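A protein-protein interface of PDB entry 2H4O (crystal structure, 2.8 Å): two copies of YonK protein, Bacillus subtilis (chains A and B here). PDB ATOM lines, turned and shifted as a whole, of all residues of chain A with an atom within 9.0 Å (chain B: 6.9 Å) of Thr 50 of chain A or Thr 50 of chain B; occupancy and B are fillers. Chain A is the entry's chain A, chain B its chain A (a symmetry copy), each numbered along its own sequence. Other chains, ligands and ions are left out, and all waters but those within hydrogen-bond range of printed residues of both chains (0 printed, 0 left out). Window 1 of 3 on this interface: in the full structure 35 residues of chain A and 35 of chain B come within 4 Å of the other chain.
The side-chain amide oxygen of Asn 10 of chain A lies within hydrogen-bond range of the side-chain amide nitrogen of Gln 8 of chain A, 3.0 Å away. The side-chain amide nitrogen of Gln 8 of chain B is in hydrogen-bond range of the side-chain amide oxygen of Asn 10 of chain B.
Of the printed residues of chain B, Val 11 of chain A touches Ser 48 and Ile 49. Lys 12 of chain A touches none of the printed residues of chain B. Ile 38 of chain A touches none of the printed residues of chain B. Of the printed residues of chain B, Leu 39 of chain A touches Phe 35. Thr 50 of chain A touches six residues of chain B. Printed residues of chain A within 4 Å of Ile 9 of chain B: Ile 49 (3.5 Å), Thr 50 (3.2 Å) and Val 51 (2.8 Å). Printed residues of chain A within 4 Å of Val 11 of chain B: Ser 48 and Ile 49. Of the printed residues of chain A, Ile 49 of chain B touches Ile 9 (3.5 Å), Asn 10 (3.3 Å), Val 11 (2.7 Å), Phe 35 (3.3 Å) and Thr 50 (3.1 Å). Of chain A, only His 7 (3.9 Å), Gln 8 (3.3 Å), Ile 9 (2.8 Å), Phe 42 (3.3 Å) and Ser 48 (3.4 Å) come within 4 Å of Val 51 of chain B.
N of Ile 9 of chain A lies within hydrogen-bond range of O of Val 51 of chain B (2.8 Å). The side-chain amide nitrogen (ND2) of Asn 10 of chain A is in hydrogen-bond range of the side-chain hydroxyl (OG1) of Thr 50 of chain B. The backbone NH (N) of Ile 49 of chain B lies within hydrogen-bond range of the backbone carbonyl oxygen (O) of Val 11 of chain A, at 2.7 Å. The backbone carbonyl oxygen (O) of Lys 52 of chain B is in hydrogen-bond range of the backbone NH (N) of Ser 48 of chain A, 2.8 Å away. N of Ile 49 of chain A is in hydrogen-bond range of O of Val 11 of chain B (2.7 Å). ND2 of Asn 10 of chain B sits at hydrogen-bond distance from OG1 of Thr 50 of chain A (3.5 Å). The backbone NH (N) of Thr 50 of chain A lies within hydrogen-bond range of the backbone carbonyl oxygen (O) of Thr 50 of chain B, at 2.7 Å. The backbone NH (N) of Ile 9 of chain B sits at hydrogen-bond distance from the backbone carbonyl oxygen (O) of Val 51 of chain A, 2.8 Å away. The backbone carbonyl oxygen (O) of Lys 52 of chain A is in hydrogen-bond range of the backbone NH (N) of Ser 48 of chain B (2.8 Å). The backbone carbonyl oxygen (O) of Ser 48 of chain A lies close to the backbone carbonyl oxygen (O) of Thr 50 of chain B (3.3 Å). The backbone carbonyl oxygen (O) of Ser 48 of chain B lies close to the backbone carbonyl oxygen (O) of Thr 50 of chain A.
Ile 9 of chain A touches Ile 49 of chain B, and with the chains exchanged Ile 49 of chain A touches Ile 9 of chain B. Asn 10 of chain A touches Thr 50 of chain B, and with the chains exchanged Thr 50 of chain A touches Asn 10 of chain B. Val 11 of chain A touches Ser 48 of chain B, and with the chains exchanged Ser 48 of chain A touches Val 11 of chain B. Ser 48 of chain A touches Val 51 of chain B, and with the chains exchanged Val 51 of chain A touches Ser 48 of chain B. Positions printed for both chains: 8, 9, 10, 11, 35, 48, 49, 50, 51 and 52.
Gln 8 of chain A touches Val 51 of chain B. Gln 8 of chain A touches Lys 52 of chain B (OE1 to CG, 3.7 Å). Ile 49 of chain B touches Asn 10 of chain A. Phe 35 of chain A touches Ile 49 of chain B. CD1 of Phe 42 of chain A touches CG1 of Val 51 of chain B, 3.3 Å away. O of Lys 52 of chain B touches CA of Val 47 of chain A, at 3.1 Å. Asn 10 of chain B touches Ile 49 of chain A. CD1 of Ile 49 of chain A touches CZ of Phe 35 of chain B, 3.3 Å away. O of Thr 50 of chain B touches CA of Ile 49 of chain A (3.1 Å). OG1 of Thr 50 of chain A touches NE2 of Gln 8 of chain B, at 3.7 Å.
Of the 10 printed residues of chain B, 10 touch a printed residue of chain A. Printed residues of chain B that touch a printed residue of chain A: Gln 8, Ile 9, Asn 10, Val 11, Phe 35, Ser 48, Ile 49, Thr 50, Val 51 and Lys 52. Of the 18 printed residues of chain A, 15 touch a printed residue of chain B. Along chain A the printed residues that touch a printed residue of chain B span positions 6 to 52. Among the printed residues, no Asp or Glu carboxylate lies within 4 Å of a Lys or Arg side-chain nitrogen of the other chain.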
ATOM      1  N   VAL A   6     -17.649  -4.970 -32.076  1.00  0.00           N
ATOM      2  CA  VAL A   6     -17.962  -4.209 -30.894  1.00  0.00           C
ATOM      3  C   VAL A   6     -19.472  -3.947 -30.851  1.00  0.00           C
ATOM      4  O   VAL A   6     -20.113  -3.796 -31.879  1.00  0.00           O
ATOM      5  CB  VAL A   6     -17.168  -2.907 -30.870  1.00  0.00           C
ATOM      6  CG2 VAL A   6     -17.750  -1.997 -29.874  1.00  0.00           C
ATOM      7  N   HIS A   7     -20.050  -3.967 -29.656  1.00  0.00           N
ATOM      8  CA  HIS A   7     -21.473  -3.701 -29.470  1.00  0.00           C
ATOM      9  C   HIS A   7     -21.517  -2.759 -28.282  1.00  0.00           C
ATOM     10  O   HIS A   7     -21.100  -3.112 -27.197  1.00  0.00           O
ATOM     11  CB  HIS A   7     -22.232  -4.977 -29.146  1.00  0.00           C
ATOM     12  CG  HIS A   7     -23.626  -4.733 -28.654  1.00  0.00           C
ATOM     13  ND1 HIS A   7     -24.509  -3.894 -29.298  1.00  0.00           N
ATOM     14  CD2 HIS A   7     -24.290  -5.214 -27.573  1.00  0.00           C
ATOM     15  CE1 HIS A   7     -25.658  -3.862 -28.638  1.00  0.00           C
ATOM     16  NE2 HIS A   7     -25.549  -4.656 -27.589  1.00  0.00           N
ATOM     17  N   GLN A   8     -22.030  -1.560 -28.476  1.00  0.00           N
ATOM     18  CA  GLN A   8     -22.026  -0.600 -27.405  1.00  0.00           C
ATOM     19  C   GLN A   8     -23.331   0.177 -27.198  1.00  0.00           C
ATOM     20  O   GLN A   8     -23.975   0.525 -28.167  1.00  0.00           O
ATOM     21  CB  GLN A   8     -20.886   0.372 -27.659  1.00  0.00           C
ATOM     22  CG  GLN A   8     -20.802   1.440 -26.670  1.00  0.00           C
ATOM     23  CD  GLN A   8     -19.679   2.360 -26.924  1.00  0.00           C
ATOM     24  OE1 GLN A   8     -18.612   1.956 -27.414  1.00  0.00           O
ATOM     25  NE2 GLN A   8     -19.880   3.622 -26.574  1.00  0.00           N
ATOM     26  N   ILE A   9     -23.720   0.427 -25.939  1.00  0.00           N
ATOM     27  CA  ILE A   9     -24.911   1.218 -25.635  1.00  0.00           C
ATOM     28  C   ILE A   9     -24.512   2.502 -24.880  1.00  0.00           C
ATOM     29  O   ILE A   9     -23.714   2.459 -23.936  1.00  0.00           O
ATOM     30  CB  ILE A   9     -25.907   0.431 -24.778  1.00  0.00           C
ATOM     31  CG1 ILE A   9     -26.683  -0.559 -25.641  1.00  0.00           C
ATOM     32  CG2 ILE A   9     -26.861   1.364 -24.085  1.00  0.00           C
ATOM     33  N   ASN A  10     -25.056   3.637 -25.317  1.00  0.00           N
ATOM     34  CA  ASN A  10     -24.789   4.937 -24.715  1.00  0.00           C
ATOM     35  C   ASN A  10     -26.130   5.379 -24.217  1.00  0.00           C
ATOM     36  O   ASN A  10     -27.086   5.278 -24.947  1.00  0.00           O
ATOM     37  CB  ASN A  10     -24.278   5.963 -25.750  1.00  0.00           C
ATOM     38  CG  ASN A  10     -22.909   5.603 -26.323  1.00  0.00           C
ATOM     39  OD1 ASN A  10     -22.694   4.492 -26.797  1.00  0.00           O
ATOM     40  ND2 ASN A  10     -21.977   6.553 -26.288  1.00  0.00           N
ATOM     41  N   VAL A  11     -26.195   5.868 -22.985  1.00  0.00           N
ATOM     42  CA  VAL A  11     -27.436   6.326 -22.397  1.00  0.00           C
ATOM     43  C   VAL A  11     -27.175   7.582 -21.582  1.00  0.00           C
ATOM     44  O   VAL A  11     -26.426   7.572 -20.642  1.00  0.00           O
ATOM     45  CB  VAL A  11     -28.068   5.233 -21.460  1.00  0.00           C
ATOM     46  CG1 VAL A  11     -29.571   5.433 -21.390  1.00  0.00           C
ATOM     47  N   LYS A  12     -27.814   8.670 -21.943  1.00  0.00           N
ATOM     48  CA  LYS A  12     -27.604   9.915 -21.242  1.00  0.00           C
ATOM     49  C   LYS A  12     -28.919  10.460 -20.726  1.00  0.00           C
ATOM     50  O   LYS A  12     -29.847  10.636 -21.497  1.00  0.00           O
ATOM     51  CB  LYS A  12     -26.962  10.940 -22.188  1.00  0.00           C
ATOM     52  N   PHE A  35     -32.970   1.149 -17.796  1.00  0.00           N
ATOM     53  CA  PHE A  35     -31.608   0.696 -17.657  1.00  0.00           C
ATOM     54  C   PHE A  35     -31.532  -0.796 -17.383  1.00  0.00           C
ATOM     55  O   PHE A  35     -30.551  -1.448 -17.765  1.00  0.00           O
ATOM     56  CB  PHE A  35     -30.955   1.497 -16.545  1.00  0.00           C
ATOM     57  CG  PHE A  35     -29.487   1.492 -16.603  1.00  0.00           C
ATOM     58  CD1 PHE A  35     -28.839   1.672 -17.813  1.00  0.00           C
ATOM     59  CD2 PHE A  35     -28.736   1.321 -15.448  1.00  0.00           C
ATOM     60  CE1 PHE A  35     -27.471   1.676 -17.877  1.00  0.00           C
ATOM     61  CE2 PHE A  35     -27.356   1.324 -15.502  1.00  0.00           C
ATOM     62  CZ  PHE A  35     -26.720   1.505 -16.723  1.00  0.00           C
ATOM     63  N   ILE A  38     -31.825  -2.666 -20.749  1.00  0.00           N
ATOM     64  CA  ILE A  38     -30.564  -2.381 -21.431  1.00  0.00           C
ATOM     65  C   ILE A  38     -29.406  -3.193 -20.812  1.00  0.00           C
ATOM     66  O   ILE A  38     -28.681  -3.931 -21.508  1.00  0.00           O
ATOM     67  CB  ILE A  38     -30.222  -0.871 -21.333  1.00  0.00           C
ATOM     68  CG1 ILE A  38     -31.245  -0.042 -22.127  1.00  0.00           C
ATOM     69  CG2 ILE A  38     -28.807  -0.630 -21.838  1.00  0.00           C
ATOM     70  CD1 ILE A  38     -31.132   1.421 -21.904  1.00  0.00           C
ATOM     71  N   LEU A  39     -29.256  -3.060 -19.494  1.00  0.00           N
ATOM     72  CA  LEU A  39     -28.214  -3.755 -18.765  1.00  0.00           C
ATOM     73  C   LEU A  39     -28.255  -5.242 -18.954  1.00  0.00           C
ATOM     74  O   LEU A  39     -27.231  -5.870 -19.030  1.00  0.00           O
ATOM     75  CB  LEU A  39     -28.320  -3.419 -17.288  1.00  0.00           C
ATOM     76  CG  LEU A  39     -27.088  -2.880 -16.573  1.00  0.00           C
ATOM     77  CD1 LEU A  39     -26.464  -1.762 -17.391  1.00  0.00           C
ATOM     78  CD2 LEU A  39     -27.503  -2.391 -15.204  1.00  0.00           C
ATOM     79  N   PHE A  42     -26.469  -7.339 -21.617  1.00  0.00           N
ATOM     80  CA  PHE A  42     -25.047  -7.596 -21.412  1.00  0.00           C
ATOM     81  C   PHE A  42     -24.726  -8.587 -20.287  1.00  0.00           C
ATOM     82  O   PHE A  42     -23.570  -8.981 -20.107  1.00  0.00           O
ATOM     83  CB  PHE A  42     -24.301  -6.275 -21.158  1.00  0.00           C
ATOM     84  CG  PHE A  42     -24.334  -5.314 -22.321  1.00  0.00           C
ATOM     85  CD1 PHE A  42     -25.202  -4.226 -22.324  1.00  0.00           C
ATOM     86  CD2 PHE A  42     -23.470  -5.482 -23.398  1.00  0.00           C
ATOM     87  CE1 PHE A  42     -25.204  -3.321 -23.369  1.00  0.00           C
ATOM     88  CE2 PHE A  42     -23.466  -4.579 -24.456  1.00  0.00           C
ATOM     89  CZ  PHE A  42     -24.335  -3.495 -24.439  1.00  0.00           C
ATOM     90  N   VAL A  47     -17.516  -6.899 -20.225  1.00  0.00           N
ATOM     91  CA  VAL A  47     -17.962  -5.585 -20.673  1.00  0.00           C
ATOM     92  C   VAL A  47     -16.990  -4.494 -20.235  1.00  0.00           C
ATOM     93  O   VAL A  47     -16.096  -4.734 -19.424  1.00  0.00           O
ATOM     94  CB  VAL A  47     -19.367  -5.253 -20.139  1.00  0.00           C
ATOM     95  CG1 VAL A  47     -20.347  -6.362 -20.491  1.00  0.00           C
ATOM     96  CG2 VAL A  47     -19.325  -5.029 -18.634  1.00  0.00           C
ATOM     97  N   SER A  48     -17.173  -3.295 -20.778  1.00  0.00           N
ATOM     98  CA  SER A  48     -16.660  -2.083 -20.147  1.00  0.00           C
ATOM     99  C   SER A  48     -17.782  -1.089 -19.870  1.00  0.00           C
ATOM    100  O   SER A  48     -18.524  -0.707 -20.776  1.00  0.00           O
ATOM    101  CB  SER A  48     -15.588  -1.435 -21.026  1.00  0.00           C
ATOM    102  OG  SER A  48     -14.788  -2.416 -21.662  1.00  0.00           O
ATOM    103  N   ILE A  49     -17.902  -0.674 -18.613  1.00  0.00           N
ATOM    104  CA  ILE A  49     -18.974   0.225 -18.201  1.00  0.00           C
ATOM    105  C   ILE A  49     -18.422   1.578 -17.767  1.00  0.00           C
ATOM    106  O   ILE A  49     -17.511   1.652 -16.943  1.00  0.00           O
ATOM    107  CB  ILE A  49     -19.795  -0.404 -17.060  1.00  0.00           C
ATOM    108  CG1 ILE A  49     -20.231  -1.821 -17.433  1.00  0.00           C
ATOM    109  CG2 ILE A  49     -21.003   0.463 -16.735  1.00  0.00           C
ATOM    110  CD1 ILE A  49     -21.310  -2.385 -16.535  1.00  0.00           C
ATOM    111  N   THR A  50     -18.979   2.647 -18.328  1.00  0.00           N
ATOM    112  CA  THR A  50     -18.584   4.000 -17.957  1.00  0.00           C
ATOM    113  C   THR A  50     -19.787   4.820 -17.502  1.00  0.00           C
ATOM    114  O   THR A  50     -20.788   4.918 -18.211  1.00  0.00           O
ATOM    115  CB  THR A  50     -17.882   4.699 -19.137  1.00  0.00           C
ATOM    116  OG1 THR A  50     -16.462   4.567 -18.997  1.00  0.00           O
ATOM    117  CG2 THR A  50     -18.102   6.203 -19.071  1.00  0.00           C
ATOM    118  N   VAL A  51     -19.681   5.407 -16.314  1.00  0.00           N
ATOM    119  CA  VAL A  51     -20.756   6.221 -15.764  1.00  0.00           C
ATOM    120  C   VAL A  51     -20.119   7.565 -15.426  1.00  0.00           C
ATOM    121  O   VAL A  51     -19.198   7.676 -14.607  1.00  0.00           O
ATOM    122  CB  VAL A  51     -21.367   5.549 -14.525  1.00  0.00           C
ATOM    123  CG1 VAL A  51     -22.479   6.383 -14.000  1.00  0.00           C
ATOM    124  CG2 VAL A  51     -21.876   4.152 -14.896  1.00  0.00           C
ATOM    125  N   LYS A  52     -20.604   8.592 -16.086  1.00  0.00           N
ATOM    126  CA  LYS A  52     -20.033   9.919 -15.939  1.00  0.00           C
ATOM    127  C   LYS A  52     -21.146  10.811 -15.469  1.00  0.00           C
ATOM    128  O   LYS A  52     -22.298  10.598 -15.827  1.00  0.00           O
ATOM    129  CB  LYS A  52     -19.481  10.402 -17.321  1.00  0.00           C
ATOM    130  CG  LYS A  52     -18.718  11.713 -17.336  1.00  0.00           C
ATOM    131  CD  LYS A  52     -19.060  12.567 -18.525  1.00  0.00           C
ATOM    132  CE  LYS A  52     -18.514  12.024 -19.819  1.00  0.00           C
ATOM    133  NZ  LYS A  52     -19.040  12.761 -21.025  1.00  0.00           N
ATOM    134  N   GLU A  53     -20.784  11.785 -14.650  1.00  0.00           N
ATOM    135  CA  GLU A  53     -21.706  12.755 -14.115  1.00  0.00           C
ATOM    136  C   GLU A  53     -20.952  14.059 -14.102  1.00  0.00           C
ATOM    137  O   GLU A  53     -19.971  14.171 -13.400  1.00  0.00           O
ATOM    138  CB  GLU A  53     -22.082  12.412 -12.695  1.00  0.00           C
ATOM    139  CG  GLU A  53     -22.881  13.536 -12.047  1.00  0.00           C
ATOM    140  CD  GLU A  53     -22.853  13.509 -10.521  1.00  0.00           C
ATOM    141  OE1 GLU A  53     -23.522  14.373  -9.907  1.00  0.00           O
ATOM    142  OE2 GLU A  53     -22.158  12.637  -9.934  1.00  0.00           O
ATOM    143  N   GLN B   8     -16.255  10.488 -12.952  1.00  0.00           N
ATOM    144  CA  GLN B   8     -16.518   9.345 -13.785  1.00  0.00           C
ATOM    145  C   GLN B   8     -16.018   7.999 -13.250  1.00  0.00           C
ATOM    146  O   GLN B   8     -14.953   7.949 -12.669  1.00  0.00           O
ATOM    147  CB  GLN B   8     -15.903   9.615 -15.148  1.00  0.00           C
ATOM    148  CG  GLN B   8     -16.047   8.504 -16.082  1.00  0.00           C
ATOM    149  CD  GLN B   8     -15.461   8.795 -17.402  1.00  0.00           C
ATOM    150  OE1 GLN B   8     -15.478   9.940 -17.879  1.00  0.00           O
ATOM    151  NE2 GLN B   8     -14.946   7.755 -18.042  1.00  0.00           N
ATOM    152  N   ILE B   9     -16.797   6.922 -13.433  1.00  0.00           N
ATOM    153  CA  ILE B   9     -16.382   5.583 -13.023  1.00  0.00           C
ATOM    154  C   ILE B   9     -16.260   4.667 -14.259  1.00  0.00           C
ATOM    155  O   ILE B   9     -17.144   4.649 -15.123  1.00  0.00           O
ATOM    156  CB  ILE B   9     -17.380   4.958 -12.043  1.00  0.00           C
ATOM    157  CG1 ILE B   9     -17.184   5.538 -10.646  1.00  0.00           C
ATOM    158  CG2 ILE B   9     -17.219   3.464 -12.005  1.00  0.00           C
ATOM    159  N   ASN B  10     -15.153   3.930 -14.340  1.00  0.00           N
ATOM    160  CA  ASN B  10     -14.882   3.012 -15.438  1.00  0.00           C
ATOM    161  C   ASN B  10     -14.806   1.674 -14.770  1.00  0.00           C
ATOM    162  O   ASN B  10     -14.152   1.560 -13.761  1.00  0.00           O
ATOM    163  CB  ASN B  10     -13.527   3.305 -16.121  1.00  0.00           C
ATOM    164  CG  ASN B  10     -13.499   4.654 -16.835  1.00  0.00           C
ATOM    165  OD1 ASN B  10     -13.828   5.684 -16.256  1.00  0.00           O
ATOM    166  ND2 ASN B  10     -13.092   4.651 -18.103  1.00  0.00           N
ATOM    167  N   VAL B  11     -15.468   0.671 -15.332  1.00  0.00           N
ATOM    168  CA  VAL B  11     -15.469  -0.666 -14.776  1.00  0.00           C
ATOM    169  C   VAL B  11     -15.391  -1.682 -15.904  1.00  0.00           C
ATOM    170  O   VAL B  11     -16.245  -1.747 -16.747  1.00  0.00           O
ATOM    171  CB  VAL B  11     -16.768  -0.940 -13.934  1.00  0.00           C
ATOM    172  CG1 VAL B  11     -16.479  -1.999 -12.886  1.00  0.00           C
ATOM    173  N   PHE B  35     -21.373  -3.583  -8.841  1.00  0.00           N
ATOM    174  CA  PHE B  35     -21.958  -2.579  -9.696  1.00  0.00           C
ATOM    175  C   PHE B  35     -23.083  -1.830  -9.004  1.00  0.00           C
ATOM    176  O   PHE B  35     -23.322  -0.653  -9.306  1.00  0.00           O
ATOM    177  CB  PHE B  35     -22.444  -3.262 -10.962  1.00  0.00           C
ATOM    178  CG  PHE B  35     -22.620  -2.344 -12.094  1.00  0.00           C
ATOM    179  CD1 PHE B  35     -21.659  -1.385 -12.366  1.00  0.00           C
ATOM    180  CD2 PHE B  35     -23.741  -2.433 -12.908  1.00  0.00           C
ATOM    181  CE1 PHE B  35     -21.809  -0.528 -13.423  1.00  0.00           C
ATOM    182  CE2 PHE B  35     -23.901  -1.574 -13.978  1.00  0.00           C
ATOM    183  CZ  PHE B  35     -22.929  -0.617 -14.238  1.00  0.00           C
ATOM    184  N   SER B  48     -24.060  10.138 -17.936  1.00  0.00           N
ATOM    185  CA  SER B  48     -23.900   9.402 -19.186  1.00  0.00           C
ATOM    186  C   SER B  48     -23.352   8.002 -18.934  1.00  0.00           C
ATOM    187  O   SER B  48     -22.301   7.838 -18.313  1.00  0.00           O
ATOM    188  CB  SER B  48     -22.979  10.163 -20.142  1.00  0.00           C
ATOM    189  OG  SER B  48     -23.191  11.561 -20.049  1.00  0.00           O
ATOM    190  N   ILE B  49     -24.070   6.994 -19.419  1.00  0.00           N
ATOM    191  CA  ILE B  49     -23.692   5.604 -19.192  1.00  0.00           C
ATOM    192  C   ILE B  49     -23.299   4.919 -20.496  1.00  0.00           C
ATOM    193  O   ILE B  49     -24.037   4.968 -21.481  1.00  0.00           O
ATOM    194  CB  ILE B  49     -24.844   4.836 -18.516  1.00  0.00           C
ATOM    195  CG1 ILE B  49     -25.340   5.595 -17.284  1.00  0.00           C
ATOM    196  CG2 ILE B  49     -24.397   3.432 -18.140  1.00  0.00           C
ATOM    197  CD1 ILE B  49     -26.224   4.769 -16.374  1.00  0.00           C
ATOM    198  N   THR B  50     -22.133   4.282 -20.497  1.00  0.00           N
ATOM    199  CA  THR B  50     -21.668   3.537 -21.660  1.00  0.00           C
ATOM    200  C   THR B  50     -21.351   2.089 -21.298  1.00  0.00           C
ATOM    201  O   THR B  50     -20.588   1.824 -20.371  1.00  0.00           O
ATOM    202  CB  THR B  50     -20.425   4.213 -22.271  1.00  0.00           C
ATOM    203  OG1 THR B  50     -20.826   5.067 -23.351  1.00  0.00           O
ATOM    204  CG2 THR B  50     -19.539   3.181 -22.951  1.00  0.00           C
ATOM    205  N   VAL B  51     -21.946   1.158 -22.037  1.00  0.00           N
ATOM    206  CA  VAL B  51     -21.727  -0.263 -21.798  1.00  0.00           C
ATOM    207  C   VAL B  51     -21.277  -0.837 -23.137  1.00  0.00           C
ATOM    208  O   VAL B  51     -21.989  -0.801 -24.149  1.00  0.00           O
ATOM    209  CB  VAL B  51     -23.013  -0.933 -21.290  1.00  0.00           C
ATOM    210  CG1 VAL B  51     -22.757  -2.372 -21.027  1.00  0.00           C
ATOM    211  CG2 VAL B  51     -23.487  -0.231 -20.012  1.00  0.00           C
ATOM    212  N   LYS B  52     -20.069  -1.353 -23.144  1.00  0.00           N
ATOM    213  CA  LYS B  52     -19.469  -1.852 -24.369  1.00  0.00           C
ATOM    214  C   LYS B  52     -19.135  -3.294 -24.121  1.00  0.00           C
ATOM    215  O   LYS B  52     -18.811  -3.668 -23.000  1.00  0.00           O
ATOM    216  CB  LYS B  52     -18.177  -1.030 -24.686  1.00  0.00           C
ATOM    217  CG  LYS B  52     -17.489  -1.314 -26.007  1.00  0.00           C
ATOM    218  CD  LYS B  52     -15.990  -1.351 -25.883  1.00  0.00           C
ATOM    219  CE  LYS B  52     -15.384   0.008 -25.650  1.00  0.00           C
ATOM    220  NZ  LYS B  52     -13.917  -0.062 -25.313  1.00  0.00           N
